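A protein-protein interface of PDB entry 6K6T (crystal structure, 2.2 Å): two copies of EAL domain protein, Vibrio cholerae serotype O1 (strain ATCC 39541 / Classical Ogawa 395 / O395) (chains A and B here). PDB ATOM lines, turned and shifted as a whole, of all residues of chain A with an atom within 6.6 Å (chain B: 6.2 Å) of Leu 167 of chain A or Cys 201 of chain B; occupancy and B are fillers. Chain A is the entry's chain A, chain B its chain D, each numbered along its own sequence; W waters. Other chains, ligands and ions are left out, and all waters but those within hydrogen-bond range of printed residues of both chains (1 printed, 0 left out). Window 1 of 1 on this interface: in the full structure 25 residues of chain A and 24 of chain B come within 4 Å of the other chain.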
ATOM      1  N   PHE A 160     -19.559  23.271  27.573  1.00  0.00           N
ATOM      2  CA  PHE A 160     -20.214  22.392  26.611  1.00  0.00           C
ATOM      3  C   PHE A 160     -21.709  22.277  26.905  1.00  0.00           C
ATOM      4  O   PHE A 160     -22.110  21.972  28.031  1.00  0.00           O
ATOM      5  CB  PHE A 160     -19.575  21.006  26.621  1.00  0.00           C
ATOM      6  CG  PHE A 160     -20.249  20.018  25.713  1.00  0.00           C
ATOM      7  CD1 PHE A 160     -19.920  19.951  24.375  1.00  0.00           C
ATOM      8  CD2 PHE A 160     -21.247  19.178  26.198  1.00  0.00           C
ATOM      9  CE1 PHE A 160     -20.562  19.038  23.523  1.00  0.00           C
ATOM     10  CE2 PHE A 160     -21.900  18.271  25.370  1.00  0.00           C
ATOM     11  CZ  PHE A 160     -21.553  18.193  24.024  1.00  0.00           C
ATOM     12  N   GLY A 161     -22.522  22.531  25.884  1.00  0.00           N
ATOM     13  CA  GLY A 161     -23.954  22.430  26.018  1.00  0.00           C
ATOM     14  C   GLY A 161     -24.634  23.709  26.442  1.00  0.00           C
ATOM     15  O   GLY A 161     -25.793  23.665  26.880  1.00  0.00           O
ATOM     16  N   TYR A 164     -22.803  28.593  22.908  1.00  0.00           N
ATOM     17  CA  TYR A 164     -21.813  28.642  21.848  1.00  0.00           C
ATOM     18  C   TYR A 164     -21.133  27.299  21.610  1.00  0.00           C
ATOM     19  O   TYR A 164     -21.276  26.715  20.536  1.00  0.00           O
ATOM     20  CB  TYR A 164     -20.800  29.741  22.197  1.00  0.00           C
ATOM     21  CG  TYR A 164     -20.537  29.897  23.695  1.00  0.00           C
ATOM     22  CD1 TYR A 164     -21.368  30.682  24.495  1.00  0.00           C
ATOM     23  CD2 TYR A 164     -19.441  29.290  24.300  1.00  0.00           C
ATOM     24  CE1 TYR A 164     -21.132  30.837  25.850  1.00  0.00           C
ATOM     25  CE2 TYR A 164     -19.195  29.447  25.658  1.00  0.00           C
ATOM     26  CZ  TYR A 164     -20.046  30.220  26.422  1.00  0.00           C
ATOM     27  OH  TYR A 164     -19.810  30.375  27.765  1.00  0.00           O
ATOM     28  N   SER A 165     -20.487  26.736  22.623  1.00  0.00           N
ATOM     29  CA  SER A 165     -19.695  25.525  22.433  1.00  0.00           C
ATOM     30  C   SER A 165     -20.600  24.292  22.486  1.00  0.00           C
ATOM     31  O   SER A 165     -21.303  24.054  23.479  1.00  0.00           O
ATOM     32  CB  SER A 165     -18.547  25.437  23.445  1.00  0.00           C
ATOM     33  OG  SER A 165     -18.944  24.955  24.702  1.00  0.00           O
ATOM     34  N   GLY A 166     -20.599  23.530  21.399  1.00  0.00           N
ATOM     35  CA  GLY A 166     -21.459  22.379  21.320  1.00  0.00           C
ATOM     36  C   GLY A 166     -20.914  21.247  20.489  1.00  0.00           C
ATOM     37  O   GLY A 166     -19.694  21.090  20.323  1.00  0.00           O
ATOM     38  N   LEU A 167     -21.849  20.436  19.984  1.00  0.00           N
ATOM     39  CA  LEU A 167     -21.513  19.210  19.276  1.00  0.00           C
ATOM     40  C   LEU A 167     -20.674  19.471  18.028  1.00  0.00           C
ATOM     41  O   LEU A 167     -19.861  18.624  17.638  1.00  0.00           O
ATOM     42  CB  LEU A 167     -22.806  18.470  18.920  1.00  0.00           C
ATOM     43  CG  LEU A 167     -23.582  17.932  20.113  1.00  0.00           C
ATOM     44  CD1 LEU A 167     -25.041  17.485  19.689  1.00  0.00           C
ATOM     45  CD2 LEU A 167     -22.785  16.802  20.763  1.00  0.00           C
ATOM     46  N   ASN A 168     -20.865  20.627  17.389  1.00  0.00           N
ATOM     47  CA  ASN A 168     -20.077  20.955  16.203  1.00  0.00           C
ATOM     48  C   ASN A 168     -18.589  20.961  16.501  1.00  0.00           C
ATOM     49  O   ASN A 168     -17.787  20.656  15.609  1.00  0.00           O
ATOM     50  CB  ASN A 168     -20.481  22.315  15.624  1.00  0.00           C
ATOM     51  CG  ASN A 168     -20.284  23.466  16.610  1.00  0.00           C
ATOM     52  OD1 ASN A 168     -20.614  23.359  17.795  1.00  0.00           O
ATOM     53  ND2 ASN A 168     -19.724  24.570  16.119  1.00  0.00           N
ATOM     54  N   LEU A 169     -18.191  21.317  17.729  1.00  0.00           N
ATOM     55  CA  LEU A 169     -16.766  21.263  18.058  1.00  0.00           C
ATOM     56  C   LEU A 169     -16.304  19.817  18.150  1.00  0.00           C
ATOM     57  O   LEU A 169     -15.273  19.448  17.567  1.00  0.00           O
ATOM     58  CB  LEU A 169     -16.448  22.031  19.351  1.00  0.00           C
ATOM     59  CG  LEU A 169     -16.615  23.561  19.349  1.00  0.00           C
ATOM     60  CD1 LEU A 169     -16.343  24.157  20.721  1.00  0.00           C
ATOM     61  CD2 LEU A 169     -15.788  24.251  18.284  1.00  0.00           C
ATOM     62  N   LEU A 170     -17.071  18.971  18.850  1.00  0.00           N
ATOM     63  CA  LEU A 170     -16.669  17.576  18.984  1.00  0.00           C
ATOM     64  C   LEU A 170     -16.604  16.859  17.642  1.00  0.00           C
ATOM     65  O   LEU A 170     -15.819  15.918  17.493  1.00  0.00           O
ATOM     66  CB  LEU A 170     -17.620  16.838  19.910  1.00  0.00           C
ATOM     67  CG  LEU A 170     -17.559  17.100  21.396  1.00  0.00           C
ATOM     68  CD1 LEU A 170     -18.469  16.097  22.056  1.00  0.00           C
ATOM     69  CD2 LEU A 170     -16.184  16.862  21.844  1.00  0.00           C
ATOM     70  N   ALA A 171     -17.394  17.298  16.650  1.00  0.00           N
ATOM     71  CA  ALA A 171     -17.447  16.599  15.364  1.00  0.00           C
ATOM     72  C   ALA A 171     -16.126  16.696  14.603  1.00  0.00           C
ATOM     73  O   ALA A 171     -15.727  15.746  13.913  1.00  0.00           O
ATOM     74  CB  ALA A 171     -18.589  17.153  14.499  1.00  0.00           C
ATOM     75  N   ASP A 172     -15.449  17.842  14.683  1.00  0.00           N
ATOM     76  CA  ASP A 172     -14.212  18.025  13.932  1.00  0.00           C
ATOM     77  C   ASP A 172     -12.944  17.841  14.757  1.00  0.00           C
ATOM     78  O   ASP A 172     -11.885  17.593  14.170  1.00  0.00           O
ATOM     79  CB  ASP A 172     -14.182  19.410  13.277  1.00  0.00           C
ATOM     80  CG  ASP A 172     -15.325  19.606  12.281  1.00  0.00           C
ATOM     81  OD1 ASP A 172     -15.763  18.609  11.659  1.00  0.00           O
ATOM     82  OD2 ASP A 172     -15.762  20.766  12.105  1.00  0.00           O
ATOM     83  N   ASN A 200     -26.745  10.338  27.890  1.00  0.00           N
ATOM     84  CA  ASN A 200     -26.404  10.137  26.491  1.00  0.00           C
ATOM     85  C   ASN A 200     -25.113  10.881  26.113  1.00  0.00           C
ATOM     86  O   ASN A 200     -24.385  10.433  25.212  1.00  0.00           O
ATOM     87  CB  ASN A 200     -27.616  10.549  25.624  1.00  0.00           C
ATOM     88  CG  ASN A 200     -28.819   9.566  25.785  1.00  0.00           C
ATOM     89  OD1 ASN A 200     -28.739   8.404  25.380  1.00  0.00           O
ATOM     90  ND2 ASN A 200     -29.892  10.025  26.409  1.00  0.00           N
ATOM     91  N   CYS A 201     -24.805  12.005  26.785  1.00  0.00           N
ATOM     92  CA  CYS A 201     -23.528  12.684  26.538  1.00  0.00           C
ATOM     93  C   CYS A 201     -22.339  11.961  27.180  1.00  0.00           C
ATOM     94  O   CYS A 201     -21.231  11.950  26.617  1.00  0.00           O
ATOM     95  CB  CYS A 201     -23.595  14.127  27.010  1.00  0.00           C
ATOM     96  SG  CYS A 201     -24.534  15.169  25.898  1.00  0.00           S
ATOM     97  N   LEU A 204     -21.537   9.290  24.780  1.00  0.00           N
ATOM     98  CA  LEU A 204     -20.818   9.894  23.657  1.00  0.00           C
ATOM     99  C   LEU A 204     -19.363  10.201  24.019  1.00  0.00           C
ATOM    100  O   LEU A 204     -18.436   9.815  23.291  1.00  0.00           O
ATOM    101  CB  LEU A 204     -21.508  11.171  23.215  1.00  0.00           C
ATOM    102  CG  LEU A 204     -20.743  11.852  22.085  1.00  0.00           C
ATOM    103  CD1 LEU A 204     -20.585  10.942  20.863  1.00  0.00           C
ATOM    104  CD2 LEU A 204     -21.426  13.156  21.719  1.00  0.00           C
ATOM    105  N   PHE A 205     -19.145  10.875  25.160  1.00  0.00           N
ATOM    106  CA  PHE A 205     -17.786  11.239  25.559  1.00  0.00           C
ATOM    107  C   PHE A 205     -16.922   9.999  25.640  1.00  0.00           C
ATOM    108  O   PHE A 205     -15.813   9.961  25.097  1.00  0.00           O
ATOM    109  CB  PHE A 205     -17.768  11.959  26.919  1.00  0.00           C
ATOM    110  CG  PHE A 205     -18.521  13.263  26.938  1.00  0.00           C
ATOM    111  CD1 PHE A 205     -18.645  14.028  25.793  1.00  0.00           C
ATOM    112  CD2 PHE A 205     -19.093  13.725  28.105  1.00  0.00           C
ATOM    113  CE1 PHE A 205     -19.345  15.215  25.808  1.00  0.00           C
ATOM    114  CE2 PHE A 205     -19.783  14.904  28.127  1.00  0.00           C
ATOM    115  CZ  PHE A 205     -19.914  15.657  26.982  1.00  0.00           C
ATOM    116  N   PHE B 160     -29.772  21.984  14.904  1.00  0.00           N
ATOM    117  CA  PHE B 160     -29.274  21.427  16.148  1.00  0.00           C
ATOM    118  C   PHE B 160     -27.823  20.967  15.969  1.00  0.00           C
ATOM    119  O   PHE B 160     -27.512  20.184  15.059  1.00  0.00           O
ATOM    120  CB  PHE B 160     -30.159  20.263  16.556  1.00  0.00           C
ATOM    121  CG  PHE B 160     -29.705  19.558  17.780  1.00  0.00           C
ATOM    122  CD1 PHE B 160     -30.004  20.061  19.043  1.00  0.00           C
ATOM    123  CD2 PHE B 160     -28.992  18.378  17.689  1.00  0.00           C
ATOM    124  CE1 PHE B 160     -29.566  19.416  20.193  1.00  0.00           C
ATOM    125  CE2 PHE B 160     -28.536  17.727  18.838  1.00  0.00           C
ATOM    126  CZ  PHE B 160     -28.836  18.252  20.097  1.00  0.00           C
ATOM    127  N   GLY B 161     -26.926  21.476  16.812  1.00  0.00           N
ATOM    128  CA  GLY B 161     -25.539  21.073  16.698  1.00  0.00           C
ATOM    129  C   GLY B 161     -24.728  21.895  15.733  1.00  0.00           C
ATOM    130  O   GLY B 161     -23.714  21.407  15.222  1.00  0.00           O
ATOM    131  N   GLY B 163     -23.309  24.779  16.604  1.00  0.00           N
ATOM    132  CA  GLY B 163     -22.754  25.790  17.480  1.00  0.00           C
ATOM    133  C   GLY B 163     -23.775  26.541  18.279  1.00  0.00           C
ATOM    134  O   GLY B 163     -23.665  26.603  19.504  1.00  0.00           O
ATOM    135  N   LEU B 167     -27.842  21.706  23.071  1.00  0.00           N
ATOM    136  CA  LEU B 167     -28.396  20.981  24.205  1.00  0.00           C
ATOM    137  C   LEU B 167     -29.077  21.911  25.191  1.00  0.00           C
ATOM    138  O   LEU B 167     -30.089  21.529  25.810  1.00  0.00           O
ATOM    139  CB  LEU B 167     -27.271  20.198  24.871  1.00  0.00           C
ATOM    140  CG  LEU B 167     -26.776  19.064  23.970  1.00  0.00           C
ATOM    141  CD1 LEU B 167     -25.385  18.517  24.401  1.00  0.00           C
ATOM    142  CD2 LEU B 167     -27.836  17.957  24.039  1.00  0.00           C
ATOM    143  N   VAL B 180     -31.410  18.032  12.642  1.00  0.00           N
ATOM    144  CA  VAL B 180     -29.974  17.954  12.885  1.00  0.00           C
ATOM    145  C   VAL B 180     -29.257  18.730  11.796  1.00  0.00           C
ATOM    146  O   VAL B 180     -29.484  18.490  10.605  1.00  0.00           O
ATOM    147  CB  VAL B 180     -29.514  16.493  12.915  1.00  0.00           C
ATOM    148  CG1 VAL B 180     -27.992  16.406  13.237  1.00  0.00           C
ATOM    149  CG2 VAL B 180     -30.352  15.718  13.913  1.00  0.00           C
ATOM    150  N   LEU B 184     -23.283  18.038  10.760  1.00  0.00           N
ATOM    151  CA  LEU B 184     -23.199  16.795  11.510  1.00  0.00           C
ATOM    152  C   LEU B 184     -23.486  15.566  10.664  1.00  0.00           C
ATOM    153  O   LEU B 184     -23.107  14.458  11.052  1.00  0.00           O
ATOM    154  CB  LEU B 184     -24.192  16.812  12.677  1.00  0.00           C
ATOM    155  CG  LEU B 184     -23.936  17.664  13.915  1.00  0.00           C
ATOM    156  CD1 LEU B 184     -24.997  17.413  14.998  1.00  0.00           C
ATOM    157  CD2 LEU B 184     -22.532  17.371  14.468  1.00  0.00           C
ATOM    158  N   SER B 196     -20.800   8.488  16.067  1.00  0.00           N
ATOM    159  CA  SER B 196     -21.070   8.408  17.505  1.00  0.00           C
ATOM    160  C   SER B 196     -21.975   9.523  17.963  1.00  0.00           C
ATOM    161  O   SER B 196     -22.879   9.289  18.773  1.00  0.00           O
ATOM    162  CB  SER B 196     -19.778   8.422  18.314  1.00  0.00           C
ATOM    163  OG  SER B 196     -19.118   7.185  18.170  1.00  0.00           O
ATOM    164  N   ILE B 197     -21.753  10.740  17.467  1.00  0.00           N
ATOM    165  CA  ILE B 197     -22.632  11.851  17.821  1.00  0.00           C
ATOM    166  C   ILE B 197     -24.092  11.514  17.493  1.00  0.00           C
ATOM    167  O   ILE B 197     -24.981  11.631  18.344  1.00  0.00           O
ATOM    168  CB  ILE B 197     -22.189  13.129  17.092  1.00  0.00           C
ATOM    169  CG1 ILE B 197     -20.844  13.644  17.609  1.00  0.00           C
ATOM    170  CG2 ILE B 197     -23.245  14.195  17.228  1.00  0.00           C
ATOM    171  CD1 ILE B 197     -20.281  14.806  16.751  1.00  0.00           C
ATOM    172  N   MET B 198     -24.355  11.056  16.260  1.00  0.00           N
ATOM    173  CA  MET B 198     -25.738  10.820  15.821  1.00  0.00           C
ATOM    174  C   MET B 198     -26.399   9.724  16.643  1.00  0.00           C
ATOM    175  O   MET B 198     -27.475   9.938  17.202  1.00  0.00           O
ATOM    176  CB  MET B 198     -25.755  10.463  14.329  1.00  0.00           C
ATOM    177  CG  MET B 198     -27.121  10.304  13.686  1.00  0.00           C
ATOM    178  SD  MET B 198     -28.099  11.821  13.588  1.00  0.00           S
ATOM    179  CE  MET B 198     -26.875  13.015  13.083  1.00  0.00           C
ATOM    180  N   LYS B 199     -25.708   8.589  16.826  1.00  0.00           N
ATOM    181  CA  LYS B 199     -26.268   7.480  17.595  1.00  0.00           C
ATOM    182  C   LYS B 199     -26.681   7.923  18.978  1.00  0.00           C
ATOM    183  O   LYS B 199     -27.775   7.583  19.451  1.00  0.00           O
ATOM    184  CB  LYS B 199     -25.270   6.327  17.722  1.00  0.00           C
ATOM    185  CG  LYS B 199     -25.612   5.458  18.971  1.00  0.00           C
ATOM    186  CD  LYS B 199     -24.628   4.310  19.296  1.00  0.00           C
ATOM    187  CE  LYS B 199     -24.832   3.825  20.751  1.00  0.00           C
ATOM    188  NZ  LYS B 199     -24.269   4.749  21.894  1.00  0.00           N
ATOM    189  N   ASN B 200     -25.822   8.687  19.653  1.00  0.00           N
ATOM    190  CA  ASN B 200     -26.180   9.070  21.014  1.00  0.00           C
ATOM    191  C   ASN B 200     -27.204  10.191  21.026  1.00  0.00           C
ATOM    192  O   ASN B 200     -27.985  10.292  21.976  1.00  0.00           O
ATOM    193  CB  ASN B 200     -24.935   9.420  21.824  1.00  0.00           C
ATOM    194  CG  ASN B 200     -24.039   8.196  22.073  1.00  0.00           C
ATOM    195  OD1 ASN B 200     -24.436   7.250  22.752  1.00  0.00           O
ATOM    196  ND2 ASN B 200     -22.845   8.211  21.507  1.00  0.00           N
ATOM    197  N   CYS B 201     -27.235  11.028  19.987  1.00  0.00           N
ATOM    198  CA  CYS B 201     -28.305  12.021  19.902  1.00  0.00           C
ATOM    199  C   CYS B 201     -29.658  11.375  19.563  1.00  0.00           C
ATOM    200  O   CYS B 201     -30.690  11.779  20.110  1.00  0.00           O
ATOM    201  CB  CYS B 201     -27.941  13.097  18.881  1.00  0.00           C
ATOM    202  SG  CYS B 201     -26.662  14.293  19.437  1.00  0.00           S
ATOM    203  N   LEU B 202     -29.677  10.358  18.689  1.00  0.00           N
ATOM    204  CA  LEU B 202     -30.936   9.651  18.420  1.00  0.00           C
ATOM    205  C   LEU B 202     -31.491   9.003  19.682  1.00  0.00           C
ATOM    206  O   LEU B 202     -32.698   9.080  19.951  1.00  0.00           O
ATOM    207  CB  LEU B 202     -30.737   8.603  17.327  1.00  0.00           C
ATOM    208  CG  LEU B 202     -30.502   9.220  15.948  1.00  0.00           C
ATOM    209  CD1 LEU B 202     -30.005   8.161  14.971  1.00  0.00           C
ATOM    210  CD2 LEU B 202     -31.765   9.852  15.383  1.00  0.00           C
ATOM    211  N   LYS B 203     -30.629   8.369  20.480  1.00  0.00           N
ATOM    212  CA  LYS B 203     -31.096   7.789  21.734  1.00  0.00           C
ATOM    213  C   LYS B 203     -31.609   8.882  22.662  1.00  0.00           C
ATOM    214  O   LYS B 203     -32.620   8.698  23.354  1.00  0.00           O
ATOM    215  CB  LYS B 203     -29.988   6.969  22.398  1.00  0.00           C
ATOM    216  CG  LYS B 203     -29.662   5.675  21.633  1.00  0.00           C
ATOM    217  CD  LYS B 203     -28.390   4.966  22.111  1.00  0.00           C
ATOM    218  CE  LYS B 203     -28.478   4.581  23.566  1.00  0.00           C
ATOM    219  NZ  LYS B 203     -28.048   3.174  23.802  1.00  0.00           N
ATOM    220  N   LEU B 204     -30.954  10.045  22.646  1.00  0.00           N
ATOM    221  CA  LEU B 204     -31.429  11.182  23.418  1.00  0.00           C
ATOM    222  C   LEU B 204     -32.797  11.623  22.908  1.00  0.00           C
ATOM    223  O   LEU B 204     -33.723  11.837  23.695  1.00  0.00           O
ATOM    224  CB  LEU B 204     -30.410  12.328  23.330  1.00  0.00           C
ATOM    225  CG  LEU B 204     -30.449  13.586  24.238  1.00  0.00           C
ATOM    226  CD1 LEU B 204     -30.271  14.966  23.536  1.00  0.00           C
ATOM    227  CD2 LEU B 204     -31.558  13.601  25.234  1.00  0.00           C
ATOM    228  N   PHE B 205     -32.932  11.789  21.585  1.00  0.00           N
ATOM    229  CA  PHE B 205     -34.203  12.227  21.010  1.00  0.00           C
ATOM    230  C   PHE B 205     -35.311  11.251  21.367  1.00  0.00           C
ATOM    231  O   PHE B 205     -36.371  11.652  21.860  1.00  0.00           O
ATOM    232  CB  PHE B 205     -34.082  12.370  19.493  1.00  0.00           C
ATOM    233  CG  PHE B 205     -33.091  13.416  19.057  1.00  0.00           C
ATOM    234  CD1 PHE B 205     -32.865  14.538  19.820  1.00  0.00           C
ATOM    235  CD2 PHE B 205     -32.363  13.247  17.886  1.00  0.00           C
ATOM    236  CE1 PHE B 205     -31.936  15.480  19.410  1.00  0.00           C
ATOM    237  CE2 PHE B 205     -31.454  14.180  17.467  1.00  0.00           C
ATOM    238  CZ  PHE B 205     -31.229  15.302  18.222  1.00  0.00           C
ATOM    239  N   SER B 206     -35.034   9.955  21.221  1.00  0.00           N
ATOM    240  CA  SER B 206     -36.030   8.949  21.562  1.00  0.00           C
ATOM    241  C   SER B 206     -36.397   9.021  23.040  1.00  0.00           C
ATOM    242  O   SER B 206     -37.570   8.850  23.396  1.00  0.00           O
ATOM    243  CB  SER B 206     -35.523   7.563  21.172  1.00  0.00           C
ATOM    244  OG  SER B 206     -36.377   6.569  21.675  1.00  0.00           O
HETATM  245  O   HOH W   1     -26.397   7.088  24.527  1.00  0.00           O
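Among the printed residues, pairs that only touch across the chains: Phe 160 of chain A with Leu 167 of chain B (3.6 Å), Leu 167 of chain A with Phe 160 of chain B (3.6 Å), Leu 167 of chain A with Ile 197 of chain B (3.9 Å), Leu 167 of chain A with Cys 201 of chain B (3.6 Å), Asn 168 of chain A with Gly 161 of chain B (3.4 Å), Ala 171 of chain A with Leu 184 of chain B (3.9 Å), Ala 171 of chain A with Ile 197 of chain B (3.6 Å), Asn 200 of chain A with Asn 200 of chain B (3.6 Å), Asn 200 of chain A with Lys 203 of chain B (3.5 Å), Asn 200 of chain A with Leu 204 of chain B (3.6 Å), Cys 201 of chain A with Leu 167 of chain B (3.8 Å), Leu 204 of chain A with Ser 196 of chain B (3.5 Å), Leu 204 of chain A with Ile 197 of chain B (3.6 Å) and Leu 204 of chain A with Asn 200 of chain B (3.4 Å).
O of Tyr 164 of chain A sits close to O of Gly 163 of chain B, 2.6 Å away. The backbone NH (N) of Gly 163 of chain B lies close to the side-chain amide oxygen (OD1) of Asn 168 of chain A (3.3 Å).
Hydrophobic or aromatic side chains of chain B that line the printed part of chain A: Phe 160, Leu 167, Leu 184, Ile 197 and Leu 204. Of the 15 printed residues of chain A, 8 touch a printed residue of chain B. Among the printed residues, 16 pairs touch across the chains. Among the printed residues, no Asp or Glu carboxylate lies within 4 Å of a Lys or Arg side-chain nitrogen of the other chain.
Water W1 lies within hydrogen-bond range of OD1 of Asn 200 of chain B and OD1 of Asn 200 of chain A.
Phe 160 of chain A touches Leu 167 of chain B, and with the chains exchanged Leu 167 of chain A touches Phe 160 of chain B. Leu 167 of chain A touches Cys 201 of chain B, and with the chains exchanged Cys 201 of chain A touches Leu 167 of chain B. Asn 200 of chain A touches its own counterpart, Asn 200 of chain B. Asn 200 of chain A touches Leu 204 of chain B, and with the chains exchanged Leu 204 of chain A touches Asn 200 of chain B. Positions printed for both chains: 160, 161, 167, 200, 201, 204 and 205. Of the 16 pairs that touch across the chains among the printed residues, 7 have their exchanged pair printed and touching as well.
The side-chain sulfur (SG) of Cys 201 of chain B lies within hydrogen-bond range of the backbone carbonyl oxygen (O) of Ile 197 of chain B (3.3 Å). NZ of Lys 199 of chain B is in hydrogen-bond range of OD1 of Asn 200 of chain B (2.6 Å). O of Ser 196 of chain B lies within hydrogen-bond range of ND2 of Asn 200 of chain B (2.9 Å). The side-chain hydroxyl (OG) of Ser 165 of chain A sits at hydrogen-bond distance from the backbone NH (N) of Phe 160 of chain A.
Of the printed residues of chain B, Phe 160 of chain A touches Leu 167 (3.6 Å). Leu 167 of chain A touches just these residues of chain B: Phe 160, Ile 197 and Cys 201. Of the printed residues of chain B, Asn 168 of chain A touches Gly 161 (3.4 Å) and Gly 163 (3.3 Å). Leu 169 of chain A touches none of the printed residues of chain B. Of the printed residues of chain A, Leu 184 of chain B touches Ala 171 (3.9 Å). Of the printed residues of chain A, Ser 196 of chain B touches Leu 204 (3.5 Å). Of the printed residues of chain A, Cys 201 of chain B touches Leu 167 (3.6 Å). Of the printed residues of chain A, Lys 203 of chain B touches Asn 200. The nearest residue of chain A that does not touch Cys 201 of chain B is Asn 200 of chain A (5.7 Å). The nearest printed residue of chain B that does not touch Asn 168 of chain A is Leu 184 of chain B (4.7 Å).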
